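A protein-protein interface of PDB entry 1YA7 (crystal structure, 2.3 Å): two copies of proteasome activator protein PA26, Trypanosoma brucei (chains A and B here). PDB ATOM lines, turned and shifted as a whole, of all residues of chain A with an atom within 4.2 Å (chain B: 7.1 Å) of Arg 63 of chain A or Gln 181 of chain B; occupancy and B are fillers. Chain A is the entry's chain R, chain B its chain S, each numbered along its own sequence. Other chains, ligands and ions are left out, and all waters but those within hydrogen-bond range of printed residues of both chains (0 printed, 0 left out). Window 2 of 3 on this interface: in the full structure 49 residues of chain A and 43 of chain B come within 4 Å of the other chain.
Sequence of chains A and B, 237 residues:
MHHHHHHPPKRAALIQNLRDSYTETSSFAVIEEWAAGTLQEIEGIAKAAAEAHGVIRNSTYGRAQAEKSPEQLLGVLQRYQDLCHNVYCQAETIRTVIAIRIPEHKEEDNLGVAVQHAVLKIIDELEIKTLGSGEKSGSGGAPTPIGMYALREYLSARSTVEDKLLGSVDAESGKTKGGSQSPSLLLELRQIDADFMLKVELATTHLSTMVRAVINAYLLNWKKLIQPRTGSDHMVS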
ATOM      1  N   GLY A  62     -13.786 -18.260   9.614  1.00  0.00           N
ATOM      2  CA  GLY A  62     -12.542 -18.533   8.916  1.00  0.00           C
ATOM      3  C   GLY A  62     -12.890 -18.915   7.499  1.00  0.00           C
ATOM      4  O   GLY A  62     -14.076 -18.914   7.132  1.00  0.00           O
ATOM      5  N   ARG A  63     -11.878 -19.265   6.706  1.00  0.00           N
ATOM      6  CA  ARG A  63     -12.118 -19.614   5.304  1.00  0.00           C
ATOM      7  C   ARG A  63     -12.955 -20.900   5.146  1.00  0.00           C
ATOM      8  O   ARG A  63     -13.484 -21.165   4.059  1.00  0.00           O
ATOM      9  CB  ARG A  63     -10.817 -19.578   4.451  1.00  0.00           C
ATOM     10  CG  ARG A  63     -10.286 -20.909   3.888  1.00  0.00           C
ATOM     11  CD  ARG A  63      -9.203 -20.731   2.785  1.00  0.00           C
ATOM     12  NE  ARG A  63      -9.344 -21.720   1.708  1.00  0.00           N
ATOM     13  CZ  ARG A  63      -8.962 -21.527   0.437  1.00  0.00           C
ATOM     14  NH1 ARG A  63      -8.405 -20.379   0.057  1.00  0.00           N
ATOM     15  NH2 ARG A  63      -9.138 -22.490  -0.463  1.00  0.00           N
ATOM     16  N   ALA A  64     -13.121 -21.655   6.235  1.00  0.00           N
ATOM     17  CA  ALA A  64     -13.988 -22.840   6.234  1.00  0.00           C
ATOM     18  C   ALA A  64     -15.483 -22.487   6.091  1.00  0.00           C
ATOM     19  O   ALA A  64     -16.285 -23.301   5.618  1.00  0.00           O
ATOM     20  CB  ALA A  64     -13.763 -23.666   7.500  1.00  0.00           C
ATOM     21  N   GLN A  65     -15.853 -21.289   6.537  1.00  0.00           N
ATOM     22  CA  GLN A  65     -17.202 -20.773   6.355  1.00  0.00           C
ATOM     23  C   GLN A  65     -17.438 -20.355   4.890  1.00  0.00           C
ATOM     24  O   GLN A  65     -18.585 -20.270   4.458  1.00  0.00           O
ATOM     25  CB  GLN A  65     -17.463 -19.594   7.303  1.00  0.00           C
ATOM     26  CG  GLN A  65     -17.841 -19.977   8.733  1.00  0.00           C
ATOM     27  CD  GLN A  65     -16.826 -20.913   9.383  1.00  0.00           C
ATOM     28  OE1 GLN A  65     -17.098 -22.098   9.543  1.00  0.00           O
ATOM     29  NE2 GLN A  65     -15.649 -20.395   9.715  1.00  0.00           N
ATOM     30  N   ALA A  66     -16.358 -20.088   4.145  1.00  0.00           N
ATOM     31  CA  ALA A  66     -16.456 -19.781   2.723  1.00  0.00           C
ATOM     32  C   ALA A  66     -16.516 -21.071   1.927  1.00  0.00           C
ATOM     33  O   ALA A  66     -16.800 -21.063   0.734  1.00  0.00           O
ATOM     34  CB  ALA A  66     -15.295 -18.928   2.270  1.00  0.00           C
ATOM     35  N   GLU A  67     -16.265 -22.184   2.594  1.00  0.00           N
ATOM     36  CA  GLU A  67     -16.163 -23.455   1.909  1.00  0.00           C
ATOM     37  C   GLU A  67     -17.489 -24.191   1.883  1.00  0.00           C
ATOM     38  O   GLU A  67     -17.689 -25.103   1.095  1.00  0.00           O
ATOM     39  CB  GLU A  67     -15.055 -24.316   2.524  1.00  0.00           C
ATOM     40  CG  GLU A  67     -13.699 -24.044   1.897  1.00  0.00           C
ATOM     41  CD  GLU A  67     -12.533 -24.535   2.733  1.00  0.00           C
ATOM     42  OE1 GLU A  67     -12.687 -25.549   3.445  1.00  0.00           O
ATOM     43  OE2 GLU A  67     -11.456 -23.894   2.670  1.00  0.00           O
ATOM     44  N   LEU A 165     -12.406 -15.079  -1.497  1.00  0.00           N
ATOM     45  CA  LEU A 165     -11.767 -15.684  -0.323  1.00  0.00           C
ATOM     46  C   LEU A 165     -11.068 -17.008  -0.622  1.00  0.00           C
ATOM     47  O   LEU A 165     -10.046 -17.327  -0.009  1.00  0.00           O
ATOM     48  CB  LEU A 165     -12.794 -15.910   0.805  1.00  0.00           C
ATOM     49  CG  LEU A 165     -13.281 -14.688   1.583  1.00  0.00           C
ATOM     50  CD1 LEU A 165     -14.420 -15.069   2.515  1.00  0.00           C
ATOM     51  CD2 LEU A 165     -12.145 -14.070   2.360  1.00  0.00           C
ATOM     52  N   LEU A 166     -11.639 -17.782  -1.540  1.00  0.00           N
ATOM     53  CA  LEU A 166     -11.119 -19.085  -1.902  1.00  0.00           C
ATOM     54  C   LEU A 166     -10.042 -18.973  -2.970  1.00  0.00           C
ATOM     55  O   LEU A 166      -9.103 -19.772  -2.989  1.00  0.00           O
ATOM     56  CB  LEU A 166     -12.254 -20.016  -2.362  1.00  0.00           C
ATOM     57  CG  LEU A 166     -13.309 -20.379  -1.312  1.00  0.00           C
ATOM     58  CD1 LEU A 166     -14.203 -21.484  -1.820  1.00  0.00           C
ATOM     59  CD2 LEU A 166     -12.656 -20.806  -0.016  1.00  0.00           C
ATOM     60  N   GLY A 167     -10.168 -17.965  -3.833  1.00  0.00           N
ATOM     61  CA  GLY A 167      -9.279 -17.800  -4.985  1.00  0.00           C
ATOM     62  C   GLY A 167      -9.322 -19.030  -5.875  1.00  0.00           C
ATOM     63  O   GLY A 167      -8.319 -19.447  -6.477  1.00  0.00           O
ATOM     64  N   LYS B 164     -18.678 -19.764 -15.044  1.00  0.00           N
ATOM     65  CA  LYS B 164     -17.887 -19.651 -13.816  1.00  0.00           C
ATOM     66  C   LYS B 164     -17.625 -21.015 -13.201  1.00  0.00           C
ATOM     67  O   LYS B 164     -16.538 -21.244 -12.671  1.00  0.00           O
ATOM     68  CB  LYS B 164     -18.562 -18.756 -12.783  1.00  0.00           C
ATOM     69  CG  LYS B 164     -18.727 -17.328 -13.238  1.00  0.00           C
ATOM     70  CD  LYS B 164     -19.168 -16.432 -12.084  1.00  0.00           C
ATOM     71  CE  LYS B 164     -19.872 -15.207 -12.634  1.00  0.00           C
ATOM     72  NZ  LYS B 164     -19.344 -13.948 -12.014  1.00  0.00           N
ATOM     73  N   LEU B 165     -18.623 -21.900 -13.285  1.00  0.00           N
ATOM     74  CA  LEU B 165     -18.546 -23.264 -12.738  1.00  0.00           C
ATOM     75  C   LEU B 165     -17.667 -24.182 -13.584  1.00  0.00           C
ATOM     76  O   LEU B 165     -16.943 -25.010 -13.050  1.00  0.00           O
ATOM     77  CB  LEU B 165     -19.945 -23.884 -12.601  1.00  0.00           C
ATOM     78  CG  LEU B 165     -20.768 -23.433 -11.394  1.00  0.00           C
ATOM     79  CD1 LEU B 165     -22.221 -23.723 -11.604  1.00  0.00           C
ATOM     80  CD2 LEU B 165     -20.242 -24.085 -10.103  1.00  0.00           C
ATOM     81  N   GLY B 178      -9.755 -23.847 -14.531  1.00  0.00           N
ATOM     82  CA  GLY B 178     -10.520 -24.484 -13.418  1.00  0.00           C
ATOM     83  C   GLY B 178     -11.783 -23.707 -13.065  1.00  0.00           C
ATOM     84  O   GLY B 178     -11.778 -22.464 -13.019  1.00  0.00           O
ATOM     85  N   GLY B 179     -12.869 -24.441 -12.823  1.00  0.00           N
ATOM     86  CA  GLY B 179     -14.132 -23.835 -12.421  1.00  0.00           C
ATOM     87  C   GLY B 179     -14.099 -23.395 -10.970  1.00  0.00           C
ATOM     88  O   GLY B 179     -13.185 -23.757 -10.226  1.00  0.00           O
ATOM     89  N   SER B 180     -15.117 -22.631 -10.577  1.00  0.00           N
ATOM     90  CA  SER B 180     -15.178 -21.962  -9.275  1.00  0.00           C
ATOM     91  C   SER B 180     -15.337 -22.934  -8.108  1.00  0.00           C
ATOM     92  O   SER B 180     -16.012 -23.960  -8.226  1.00  0.00           O
ATOM     93  CB  SER B 180     -16.315 -20.931  -9.286  1.00  0.00           C
ATOM     94  OG  SER B 180     -16.415 -20.218  -8.066  1.00  0.00           O
ATOM     95  N   GLN B 181     -14.703 -22.592  -6.985  1.00  0.00           N
ATOM     96  CA  GLN B 181     -14.749 -23.388  -5.755  1.00  0.00           C
ATOM     97  C   GLN B 181     -15.982 -23.052  -4.906  1.00  0.00           C
ATOM     98  O   GLN B 181     -16.325 -23.788  -3.961  1.00  0.00           O
ATOM     99  CB  GLN B 181     -13.475 -23.163  -4.898  1.00  0.00           C
ATOM    100  CG  GLN B 181     -12.108 -23.467  -5.571  1.00  0.00           C
ATOM    101  CD  GLN B 181     -10.896 -23.090  -4.679  1.00  0.00           C
ATOM    102  OE1 GLN B 181     -10.266 -22.049  -4.893  1.00  0.00           O
ATOM    103  NE2 GLN B 181     -10.597 -23.918  -3.674  1.00  0.00           N
ATOM    104  N   SER B 182     -16.645 -21.944  -5.251  1.00  0.00           N
ATOM    105  CA  SER B 182     -17.721 -21.372  -4.427  1.00  0.00           C
ATOM    106  C   SER B 182     -18.920 -22.310  -4.283  1.00  0.00           C
ATOM    107  O   SER B 182     -19.507 -22.686  -5.291  1.00  0.00           O
ATOM    108  CB  SER B 182     -18.125 -20.013  -4.994  1.00  0.00           C
ATOM    109  OG  SER B 182     -19.444 -19.659  -4.649  1.00  0.00           O
ATOM    110  N   PRO B 183     -19.258 -22.725  -3.049  1.00  0.00           N
ATOM    111  CA  PRO B 183     -20.449 -23.563  -2.817  1.00  0.00           C
ATOM    112  C   PRO B 183     -21.792 -22.867  -3.142  1.00  0.00           C
ATOM    113  O   PRO B 183     -22.675 -23.487  -3.730  1.00  0.00           O
ATOM    114  CB  PRO B 183     -20.351 -23.928  -1.333  1.00  0.00           C
ATOM    115  CG  PRO B 183     -19.525 -22.868  -0.741  1.00  0.00           C
ATOM    116  CD  PRO B 183     -18.522 -22.469  -1.796  1.00  0.00           C
ATOM    117  N   SER B 184     -21.934 -21.592  -2.786  1.00  0.00           N
ATOM    118  CA  SER B 184     -23.152 -20.825  -3.110  1.00  0.00           C
ATOM    119  C   SER B 184     -23.391 -20.688  -4.624  1.00  0.00           C
ATOM    120  O   SER B 184     -24.537 -20.642  -5.061  1.00  0.00           O
ATOM    121  CB  SER B 184     -23.115 -19.446  -2.460  1.00  0.00           C
ATOM    122  OG  SER B 184     -22.995 -19.553  -1.060  1.00  0.00           O
ATOM    123  N   LEU B 185     -22.321 -20.652  -5.417  1.00  0.00           N
ATOM    124  CA  LEU B 185     -22.456 -20.520  -6.865  1.00  0.00           C
ATOM    125  C   LEU B 185     -23.097 -21.740  -7.515  1.00  0.00           C
ATOM    126  O   LEU B 185     -23.835 -21.597  -8.489  1.00  0.00           O
ATOM    127  CB  LEU B 185     -21.119 -20.191  -7.532  1.00  0.00           C
ATOM    128  CG  LEU B 185     -21.132 -19.923  -9.045  1.00  0.00           C
ATOM    129  CD1 LEU B 185     -21.605 -18.505  -9.388  1.00  0.00           C
ATOM    130  CD2 LEU B 185     -19.735 -20.159  -9.599  1.00  0.00           C
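The side-chain amide oxygen of Gln 181 of chain B lies close to the backbone carbonyl oxygen of Leu 166 of chain A (3.2 Å).
The guanidinium group (NH1) of Arg 63 of chain A is in hydrogen-bond range of the backbone carbonyl oxygen (O) of Leu 166 of chain A, at 3.2 Å. The guanidinium group of Arg 63 of chain A is in hydrogen-bond range of the backbone carbonyl oxygen of Leu 165 of chain A, 3.5 Å away. The side-chain carboxylate (OE2) of Glu 67 of chain A is in salt-bridge range of the guanidinium group (NE) of Arg 63 of chain A (3.2 Å).
Position printed for both chains: 165.
Arg 63 of chain A touches just one residue of chain B: Gln 181. Of chain A, only Arg 63 (3.8 Å), Leu 166 (3.2 Å) and Gly 167 (3.3 Å) come within 4 Å of Gln 181 of chain B. Of the printed residues of chain B, Gly 167 of chain A touches Gln 181. Of the printed residues of chain B, Glu 67 of chain A touches Pro 183 (3.4 Å). Of the printed residues of chain A, Pro 183 of chain B touches Ala 66 (3.4 Å) and Glu 67 (3.4 Å). Printed residues of chain B within 4 Å of Leu 166 of chain A: Gln 181. Ser 180 of chain B touches none of the printed residues of chain A. The nearest printed residue of chain B that does not touch Arg 63 of chain A is Pro 183 of chain B (7.8 Å). The nearest printed residue of chain A that does not touch Gln 181 of chain B is Glu 67 of chain A (5.4 Å).
Hydrophobic or aromatic side chains of chain B within 4 Å of the printed part of chain A: Pro 183. Along chain B the printed residues that touch a printed residue of chain A span positions 181 to 183. Of the 9 printed residues of chain A, 5 touch a printed residue of chain B. Among the printed residues, 5 pairs touch across the chains. Among the printed residues, no Asp or Glu carboxylate lies within 4 Å of a Lys or Arg side-chain nitrogen of the other chain.
Gln 181 of chain B touches Arg 63 of chain A (NE2 to NH2, 3.8 Å). CD of Pro 183 of chain B touches O of Ala 66 of chain A, at 3.4 Å. Glu 67 of chain A touches Pro 183 of chain B (O to CG, 3.4 Å). Gln 181 of chain B touches Gly 167 of chain A.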
